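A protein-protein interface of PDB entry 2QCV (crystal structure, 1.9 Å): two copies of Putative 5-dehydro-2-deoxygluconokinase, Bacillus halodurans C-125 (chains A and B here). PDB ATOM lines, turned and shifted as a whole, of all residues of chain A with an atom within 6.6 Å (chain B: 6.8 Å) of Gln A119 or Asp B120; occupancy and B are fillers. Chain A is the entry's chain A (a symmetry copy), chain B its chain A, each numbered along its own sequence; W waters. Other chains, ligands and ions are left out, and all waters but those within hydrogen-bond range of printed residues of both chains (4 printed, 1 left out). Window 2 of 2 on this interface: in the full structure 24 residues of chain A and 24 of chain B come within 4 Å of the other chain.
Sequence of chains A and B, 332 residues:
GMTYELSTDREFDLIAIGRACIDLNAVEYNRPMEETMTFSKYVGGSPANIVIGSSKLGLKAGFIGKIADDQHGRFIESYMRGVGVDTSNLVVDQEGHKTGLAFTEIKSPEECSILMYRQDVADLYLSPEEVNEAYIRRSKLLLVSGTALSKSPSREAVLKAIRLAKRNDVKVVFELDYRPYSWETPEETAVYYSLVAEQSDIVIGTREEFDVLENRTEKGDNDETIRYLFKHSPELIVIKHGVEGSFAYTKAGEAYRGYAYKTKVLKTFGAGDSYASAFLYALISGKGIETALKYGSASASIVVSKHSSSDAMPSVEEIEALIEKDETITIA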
ATOM      1  N   HIS A  97      24.129 -13.100   8.858  1.00  0.00           N
ATOM      2  CA  HIS A  97      24.327 -12.986   7.408  1.00  0.00           C
ATOM      3  C   HIS A  97      25.394 -11.962   7.034  1.00  0.00           C
ATOM      4  O   HIS A  97      25.504 -10.918   7.648  1.00  0.00           O
ATOM      5  CB  HIS A  97      23.020 -12.652   6.698  1.00  0.00           C
ATOM      6  CG  HIS A  97      21.956 -13.683   6.907  1.00  0.00           C
ATOM      7  ND1 HIS A  97      20.751 -13.390   7.508  1.00  0.00           N
ATOM      8  CD2 HIS A  97      21.931 -15.011   6.627  1.00  0.00           C
ATOM      9  CE1 HIS A  97      20.017 -14.487   7.559  1.00  0.00           C
ATOM     10  NE2 HIS A  97      20.712 -15.485   7.043  1.00  0.00           N
ATOM     11  N   LYS A  98      26.182 -12.298   6.022  1.00  0.00           N
ATOM     12  CA  LYS A  98      27.291 -11.482   5.534  1.00  0.00           C
ATOM     13  C   LYS A  98      26.850 -10.513   4.453  1.00  0.00           C
ATOM     14  O   LYS A  98      25.855 -10.737   3.765  1.00  0.00           O
ATOM     15  CB  LYS A  98      28.372 -12.397   4.932  1.00  0.00           C
ATOM     16  CG  LYS A  98      28.880 -13.458   5.851  1.00  0.00           C
ATOM     17  CD  LYS A  98      29.696 -12.901   6.969  1.00  0.00           C
ATOM     18  CE  LYS A  98      30.076 -14.036   7.933  1.00  0.00           C
ATOM     19  NZ  LYS A  98      30.941 -13.542   8.973  1.00  0.00           N
ATOM     20  N   MET A 116      31.230 -12.455  -7.761  1.00  0.00           N
ATOM     21  CA  MET A 116      30.257 -12.065  -6.757  1.00  0.00           C
ATOM     22  C   MET A 116      30.082 -13.082  -5.644  1.00  0.00           C
ATOM     23  O   MET A 116      30.023 -14.285  -5.886  1.00  0.00           O
ATOM     24  CB  MET A 116      28.894 -11.829  -7.427  1.00  0.00           C
ATOM     25  CG  MET A 116      27.841 -11.244  -6.513  1.00  0.00           C
ATOM     26  SD  MET A 116      28.013  -9.264  -6.336  1.00  0.00           S
ATOM     27  CE  MET A 116      26.916  -8.977  -4.666  1.00  0.00           C
ATOM     28  N   TYR A 117      30.029 -12.588  -4.412  1.00  0.00           N
ATOM     29  CA  TYR A 117      29.626 -13.372  -3.246  1.00  0.00           C
ATOM     30  C   TYR A 117      28.192 -12.902  -2.940  1.00  0.00           C
ATOM     31  O   TYR A 117      28.003 -11.785  -2.483  1.00  0.00           O
ATOM     32  CB  TYR A 117      30.574 -13.090  -2.081  1.00  0.00           C
ATOM     33  CG  TYR A 117      31.882 -13.842  -2.238  1.00  0.00           C
ATOM     34  CD1 TYR A 117      32.777 -13.531  -3.262  1.00  0.00           C
ATOM     35  CD2 TYR A 117      32.198 -14.880  -1.379  1.00  0.00           C
ATOM     36  CE1 TYR A 117      33.961 -14.238  -3.402  1.00  0.00           C
ATOM     37  CE2 TYR A 117      33.380 -15.598  -1.509  1.00  0.00           C
ATOM     38  CZ  TYR A 117      34.253 -15.268  -2.524  1.00  0.00           C
ATOM     39  OH  TYR A 117      35.409 -16.000  -2.651  1.00  0.00           O
ATOM     40  N   ARG A 118      27.195 -13.721  -3.292  1.00  0.00           N
ATOM     41  CA  ARG A 118      25.760 -13.304  -3.242  1.00  0.00           C
ATOM     42  C   ARG A 118      24.847 -14.261  -2.457  1.00  0.00           C
ATOM     43  O   ARG A 118      23.693 -13.922  -2.176  1.00  0.00           O
ATOM     44  CB  ARG A 118      25.208 -13.155  -4.655  1.00  0.00           C
ATOM     45  CG  ARG A 118      25.079 -14.465  -5.377  1.00  0.00           C
ATOM     46  CD  ARG A 118      24.472 -14.307  -6.782  1.00  0.00           C
ATOM     47  NE  ARG A 118      25.433 -13.875  -7.793  1.00  0.00           N
ATOM     48  CZ  ARG A 118      26.382 -14.657  -8.303  1.00  0.00           C
ATOM     49  NH1 ARG A 118      26.552 -15.909  -7.864  1.00  0.00           N
ATOM     50  NH2 ARG A 118      27.192 -14.178  -9.241  1.00  0.00           N
ATOM     51  N   GLN A 119      25.347 -15.422  -2.060  1.00  0.00           N
ATOM     52  CA  GLN A 119      24.491 -16.413  -1.390  1.00  0.00           C
ATOM     53  C   GLN A 119      24.153 -16.047   0.056  1.00  0.00           C
ATOM     54  O   GLN A 119      25.037 -15.841   0.898  1.00  0.00           O
ATOM     55  CB  GLN A 119      25.094 -17.830  -1.436  1.00  0.00           C
ATOM     56  CG  GLN A 119      24.403 -18.829  -0.494  1.00  0.00           C
ATOM     57  CD  GLN A 119      24.987 -20.216  -0.548  1.00  0.00           C
ATOM     58  OE1 GLN A 119      25.079 -20.795  -1.617  1.00  0.00           O
ATOM     59  NE2 GLN A 119      25.383 -20.762   0.609  1.00  0.00           N
ATOM     60  N   ASP A 120      22.855 -15.994   0.357  1.00  0.00           N
ATOM     61  CA  ASP A 120      22.392 -15.727   1.726  1.00  0.00           C
ATOM     62  C   ASP A 120      22.989 -14.470   2.308  1.00  0.00           C
ATOM     63  O   ASP A 120      23.257 -14.378   3.508  1.00  0.00           O
ATOM     64  CB  ASP A 120      22.654 -16.922   2.641  1.00  0.00           C
ATOM     65  CG  ASP A 120      21.771 -18.096   2.294  1.00  0.00           C
ATOM     66  OD1 ASP A 120      20.594 -17.876   1.915  1.00  0.00           O
ATOM     67  OD2 ASP A 120      22.254 -19.233   2.380  1.00  0.00           O
ATOM     68  N   VAL A 121      23.155 -13.474   1.461  1.00  0.00           N
ATOM     69  CA  VAL A 121      23.700 -12.212   1.929  1.00  0.00           C
ATOM     70  C   VAL A 121      22.634 -11.408   2.673  1.00  0.00           C
ATOM     71  O   VAL A 121      21.416 -11.606   2.446  1.00  0.00           O
ATOM     72  CB  VAL A 121      24.392 -11.406   0.786  1.00  0.00           C
ATOM     73  CG1 VAL A 121      25.650 -12.130   0.368  1.00  0.00           C
ATOM     74  CG2 VAL A 121      23.478 -11.024  -0.407  1.00  0.00           C
ATOM     75  N   ALA A 122      23.095 -10.533   3.572  1.00  0.00           N
ATOM     76  CA  ALA A 122      22.232  -9.752   4.432  1.00  0.00           C
ATOM     77  C   ALA A 122      21.142  -8.992   3.653  1.00  0.00           C
ATOM     78  O   ALA A 122      20.010  -8.919   4.113  1.00  0.00           O
ATOM     79  CB  ALA A 122      23.056  -8.785   5.282  1.00  0.00           C
ATOM     80  N   LEU A 124      19.357  -9.578   1.197  1.00  0.00           N
ATOM     81  CA  LEU A 124      18.253 -10.405   0.734  1.00  0.00           C
ATOM     82  C   LEU A 124      17.302 -10.781   1.859  1.00  0.00           C
ATOM     83  O   LEU A 124      16.219 -11.262   1.576  1.00  0.00           O
ATOM     84  CB  LEU A 124      18.781 -11.671   0.041  1.00  0.00           C
ATOM     85  CG  LEU A 124      19.566 -11.441  -1.264  1.00  0.00           C
ATOM     86  CD1 LEU A 124      20.134 -12.804  -1.776  1.00  0.00           C
ATOM     87  CD2 LEU A 124      18.703 -10.760  -2.278  1.00  0.00           C
ATOM     88  N   TYR A 125      17.684 -10.526   3.114  1.00  0.00           N
ATOM     89  CA  TYR A 125      16.844 -10.797   4.272  1.00  0.00           C
ATOM     90  C   TYR A 125      16.025  -9.600   4.755  1.00  0.00           C
ATOM     91  O   TYR A 125      15.387  -9.688   5.783  1.00  0.00           O
ATOM     92  CB  TYR A 125      17.706 -11.381   5.405  1.00  0.00           C
ATOM     93  CG  TYR A 125      18.074 -12.788   5.052  1.00  0.00           C
ATOM     94  CD1 TYR A 125      17.176 -13.812   5.313  1.00  0.00           C
ATOM     95  CD2 TYR A 125      19.238 -13.086   4.343  1.00  0.00           C
ATOM     96  CE1 TYR A 125      17.432 -15.090   4.948  1.00  0.00           C
ATOM     97  CE2 TYR A 125      19.527 -14.407   3.972  1.00  0.00           C
ATOM     98  CZ  TYR A 125      18.610 -15.395   4.275  1.00  0.00           C
ATOM     99  OH  TYR A 125      18.831 -16.706   3.947  1.00  0.00           O
ATOM    100  N   ASP B  93      36.135 -27.250  -7.842  1.00  0.00           N
ATOM    101  CA  ASP B  93      34.721 -27.401  -7.538  1.00  0.00           C
ATOM    102  C   ASP B  93      33.911 -27.104  -8.791  1.00  0.00           C
ATOM    103  O   ASP B  93      34.175 -26.129  -9.478  1.00  0.00           O
ATOM    104  CB  ASP B  93      34.332 -26.425  -6.440  1.00  0.00           C
ATOM    105  CG  ASP B  93      32.861 -26.493  -6.066  1.00  0.00           C
ATOM    106  OD1 ASP B  93      32.027 -25.802  -6.690  1.00  0.00           O
ATOM    107  OD2 ASP B  93      32.528 -27.222  -5.106  1.00  0.00           O
ATOM    108  N   GLY B  96      29.735 -24.390  -8.304  1.00  0.00           N
ATOM    109  CA  GLY B  96      29.540 -22.958  -8.084  1.00  0.00           C
ATOM    110  C   GLY B  96      29.929 -22.463  -6.701  1.00  0.00           C
ATOM    111  O   GLY B  96      29.650 -21.342  -6.339  1.00  0.00           O
ATOM    112  N   HIS B  97      30.585 -23.290  -5.907  1.00  0.00           N
ATOM    113  CA  HIS B  97      31.003 -22.849  -4.570  1.00  0.00           C
ATOM    114  C   HIS B  97      32.167 -21.864  -4.608  1.00  0.00           C
ATOM    115  O   HIS B  97      33.073 -21.993  -5.409  1.00  0.00           O
ATOM    116  CB  HIS B  97      31.361 -24.038  -3.685  1.00  0.00           C
ATOM    117  CG  HIS B  97      30.224 -24.990  -3.489  1.00  0.00           C
ATOM    118  ND1 HIS B  97      30.289 -26.309  -3.880  1.00  0.00           N
ATOM    119  CD2 HIS B  97      28.981 -24.803  -2.975  1.00  0.00           C
ATOM    120  CE1 HIS B  97      29.146 -26.903  -3.585  1.00  0.00           C
ATOM    121  NE2 HIS B  97      28.333 -26.011  -3.046  1.00  0.00           N
ATOM    122  N   LYS B  98      32.107 -20.872  -3.730  1.00  0.00           N
ATOM    123  CA  LYS B  98      33.094 -19.800  -3.629  1.00  0.00           C
ATOM    124  C   LYS B  98      34.219 -20.153  -2.674  1.00  0.00           C
ATOM    125  O   LYS B  98      34.054 -20.973  -1.771  1.00  0.00           O
ATOM    126  CB  LYS B  98      32.412 -18.526  -3.100  1.00  0.00           C
ATOM    127  CG  LYS B  98      31.235 -18.068  -3.896  1.00  0.00           C
ATOM    128  CD  LYS B  98      31.624 -17.539  -5.236  1.00  0.00           C
ATOM    129  CE  LYS B  98      30.354 -17.204  -6.035  1.00  0.00           C
ATOM    130  NZ  LYS B  98      30.702 -16.607  -7.299  1.00  0.00           N
ATOM    131  N   THR B  99      35.355 -19.488  -2.864  1.00  0.00           N
ATOM    132  CA  THR B  99      36.491 -19.584  -1.972  1.00  0.00           C
ATOM    133  C   THR B  99      36.215 -18.892  -0.655  1.00  0.00           C
ATOM    134  O   THR B  99      35.654 -17.796  -0.628  1.00  0.00           O
ATOM    135  CB  THR B  99      37.743 -18.917  -2.629  1.00  0.00           C
ATOM    136  OG1 THR B  99      37.888 -19.362  -3.993  1.00  0.00           O
ATOM    137  CG2 THR B  99      39.043 -19.191  -1.817  1.00  0.00           C
ATOM    138  N   ARG B 118      32.664 -18.034   5.295  1.00  0.00           N
ATOM    139  CA  ARG B 118      32.941 -19.495   5.458  1.00  0.00           C
ATOM    140  C   ARG B 118      31.774 -20.412   5.057  1.00  0.00           C
ATOM    141  O   ARG B 118      31.951 -21.630   4.956  1.00  0.00           O
ATOM    142  CB  ARG B 118      33.322 -19.798   6.903  1.00  0.00           C
ATOM    143  CG  ARG B 118      32.176 -19.636   7.859  1.00  0.00           C
ATOM    144  CD  ARG B 118      32.561 -19.995   9.306  1.00  0.00           C
ATOM    145  NE  ARG B 118      33.265 -18.927  10.009  1.00  0.00           N
ATOM    146  CZ  ARG B 118      32.683 -17.814  10.452  1.00  0.00           C
ATOM    147  NH1 ARG B 118      31.388 -17.576  10.220  1.00  0.00           N
ATOM    148  NH2 ARG B 118      33.406 -16.912  11.107  1.00  0.00           N
ATOM    149  N   GLN B 119      30.602 -19.855   4.784  1.00  0.00           N
ATOM    150  CA  GLN B 119      29.429 -20.692   4.487  1.00  0.00           C
ATOM    151  C   GLN B 119      29.469 -21.326   3.097  1.00  0.00           C
ATOM    152  O   GLN B 119      29.576 -20.640   2.072  1.00  0.00           O
ATOM    153  CB  GLN B 119      28.105 -19.925   4.667  1.00  0.00           C
ATOM    154  CG  GLN B 119      26.884 -20.648   4.077  1.00  0.00           C
ATOM    155  CD  GLN B 119      25.590 -19.900   4.262  1.00  0.00           C
ATOM    156  OE1 GLN B 119      25.246 -19.549   5.377  1.00  0.00           O
ATOM    157  NE2 GLN B 119      24.859 -19.656   3.167  1.00  0.00           N
ATOM    158  N   ASP B 120      29.352 -22.655   3.056  1.00  0.00           N
ATOM    159  CA  ASP B 120      29.300 -23.384   1.782  1.00  0.00           C
ATOM    160  C   ASP B 120      30.461 -23.058   0.876  1.00  0.00           C
ATOM    161  O   ASP B 120      30.333 -23.024  -0.350  1.00  0.00           O
ATOM    162  CB  ASP B 120      27.973 -23.150   1.063  1.00  0.00           C
ATOM    163  CG  ASP B 120      26.822 -23.807   1.786  1.00  0.00           C
ATOM    164  OD1 ASP B 120      27.014 -24.915   2.347  1.00  0.00           O
ATOM    165  OD2 ASP B 120      25.735 -23.215   1.811  1.00  0.00           O
ATOM    166  N   VAL B 121      31.617 -22.865   1.479  1.00  0.00           N
ATOM    167  CA  VAL B 121      32.801 -22.569   0.693  1.00  0.00           C
ATOM    168  C   VAL B 121      33.348 -23.840   0.044  1.00  0.00           C
ATOM    169  O   VAL B 121      33.098 -24.964   0.542  1.00  0.00           O
ATOM    170  CB  VAL B 121      33.874 -21.784   1.510  1.00  0.00           C
ATOM    171  CG1 VAL B 121      33.356 -20.394   1.792  1.00  0.00           C
ATOM    172  CG2 VAL B 121      34.409 -22.509   2.773  1.00  0.00           C
ATOM    173  N   ALA B 122      34.061 -23.657  -1.071  1.00  0.00           N
ATOM    174  CA  ALA B 122      34.579 -24.749  -1.868  1.00  0.00           C
ATOM    175  C   ALA B 122      35.386 -25.764  -1.036  1.00  0.00           C
ATOM    176  O   ALA B 122      35.270 -26.961  -1.266  1.00  0.00           O
ATOM    177  CB  ALA B 122      35.422 -24.214  -3.025  1.00  0.00           C
ATOM    178  N   ASP B 123      36.226 -25.304  -0.111  1.00  0.00           N
ATOM    179  CA  ASP B 123      37.122 -26.255   0.579  1.00  0.00           C
ATOM    180  C   ASP B 123      36.384 -27.309   1.401  1.00  0.00           C
ATOM    181  O   ASP B 123      36.929 -28.378   1.645  1.00  0.00           O
ATOM    182  CB  ASP B 123      38.184 -25.563   1.387  1.00  0.00           C
ATOM    183  CG  ASP B 123      37.626 -24.775   2.570  1.00  0.00           C
ATOM    184  OD1 ASP B 123      37.296 -25.389   3.591  1.00  0.00           O
ATOM    185  OD2 ASP B 123      37.626 -23.539   2.496  1.00  0.00           O
ATOM    186  N   LEU B 124      35.155 -26.994   1.792  1.00  0.00           N
ATOM    187  CA  LEU B 124      34.347 -27.889   2.607  1.00  0.00           C
ATOM    188  C   LEU B 124      33.675 -28.975   1.781  1.00  0.00           C
ATOM    189  O   LEU B 124      33.171 -29.923   2.357  1.00  0.00           O
ATOM    190  CB  LEU B 124      33.294 -27.097   3.397  1.00  0.00           C
ATOM    191  CG  LEU B 124      33.845 -26.123   4.456  1.00  0.00           C
ATOM    192  CD1 LEU B 124      32.664 -25.312   5.081  1.00  0.00           C
ATOM    193  CD2 LEU B 124      34.640 -26.864   5.482  1.00  0.00           C
ATOM    194  N   TYR B 125      33.705 -28.858   0.450  1.00  0.00           N
ATOM    195  CA  TYR B 125      33.140 -29.854  -0.449  1.00  0.00           C
ATOM    196  C   TYR B 125      34.143 -30.885  -0.966  1.00  0.00           C
ATOM    197  O   TYR B 125      33.798 -31.682  -1.812  1.00  0.00           O
ATOM    198  CB  TYR B 125      32.416 -29.146  -1.608  1.00  0.00           C
ATOM    199  CG  TYR B 125      31.144 -28.553  -1.087  1.00  0.00           C
ATOM    200  CD1 TYR B 125      30.016 -29.354  -0.975  1.00  0.00           C
ATOM    201  CD2 TYR B 125      31.092 -27.254  -0.584  1.00  0.00           C
ATOM    202  CE1 TYR B 125      28.863 -28.884  -0.445  1.00  0.00           C
ATOM    203  CE2 TYR B 125      29.900 -26.745  -0.046  1.00  0.00           C
ATOM    204  CZ  TYR B 125      28.799 -27.576   0.023  1.00  0.00           C
ATOM    205  OH  TYR B 125      27.603 -27.143   0.530  1.00  0.00           O
HETATM  206  O   HOH W   1      33.286 -13.593  11.000  1.00  0.00           O
HETATM  207  O   HOH W   2      35.981 -17.711  -5.003  1.00  0.00           O
HETATM  208  O   HOH W   3      28.674 -17.192  -9.494  1.00  0.00           O
HETATM  209  O   HOH W   4      30.638 -15.056  11.598  1.00  0.00           O
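Tyr A117 touches Lys B98 (CE2 to CB, 3.5 Å).
Gln A119 touches its own counterpart, Gln B119. Gln A119 touches Asp B120, and with the chains exchanged Asp A120 touches Gln B119. Positions printed for both chains: 97, 98, 118, 119, 120, 121, 122, 124 and 125. Of the 6 pairs that touch across the chains among the printed residues, 3 have their exchanged pair printed and touching as well.
Water W2 lies within hydrogen-bond range of the side-chain hydroxyl (OG1) of Thr B99 (2.7 Å) and the side-chain hydroxyl (OH) of Tyr A117 (3.0 Å). Water W3 lies within hydrogen-bond range of the guanidinium group (NH1) of Arg A118 and the side-chain amino group (NZ) of Lys B98. Water W4 bridges the guanidinium group (NH1) of Arg B118 (3.0 Å) and the side-chain amino group (NZ) of Lys A98 (3.0 Å). Water W1 lies within hydrogen-bond range of the side-chain amino group (NZ) of Lys A98 (3.1 Å) and the guanidinium group (NH2) of Arg B118 (3.3 Å).
OH of Tyr A125 lies within hydrogen-bond range of OD1 of Asp A120, at 2.9 Å. The side-chain carboxylate (OD1) of Asp B120 sits at hydrogen-bond distance from the side-chain hydroxyl (OH) of Tyr B125 (2.9 Å). The backbone carbonyl oxygen (O) of Lys B98 lies within hydrogen-bond range of the backbone NH (N) of Ala B122.
NE2 of Gln B119 sits at hydrogen-bond distance from OD2 of Asp A120, 2.8 Å away. The side-chain amide nitrogen (NE2) of Gln A119 sits close to the side-chain amide nitrogen (NE2) of Gln B119 (2.8 Å). NZ of Lys B98 lies within hydrogen-bond range of O of Met A116 (2.8 Å). OH of Tyr A117 sits at hydrogen-bond distance from O of Thr B99 (2.7 Å). The side-chain carboxylate (OD2) of Asp B120 is in hydrogen-bond range of the side-chain amide nitrogen (NE2) of Gln A119 (2.8 Å).
Of the 11 printed residues of chain A, 4 touch a printed residue of chain B. Hydrophobic or aromatic side chains of chain A within 4 Å of the printed part of chain B: Tyr A117. Along chain A the printed residues that touch a printed residue of chain B span positions 116 to 120. Of the 13 printed residues of chain B, 4 touch a printed residue of chain A. Along chain B the printed residues that touch a printed residue of chain A span positions 98 to 120. Among the printed residues, no Asp or Glu carboxylate lies within 4 Å of a Lys or Arg side-chain nitrogen of the other chain.
Printed residues of chain B within 4 Å of Tyr A117: Lys B98 (3.5 Å) and Thr B99 (2.7 Å). Gln A119 touches two residues of chain B. Ala A122 touches none of the printed residues of chain B. Of the printed residues of chain A, Lys B98 touches Met A116 (2.8 Å) and Tyr A117 (3.5 Å). Arg B118 touches none of the printed residues of chain A. Asp B120 touches one residue of chain A. The nearest residue of chain B that does not touch Gln A119 is His B97 (5.8 Å). The nearest residue of chain A that does not touch Asp B120 is Asp A120 (5.3 Å). The nearest printed residue of chain B that does not touch Met A116 is Gly B96 (7.1 Å).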
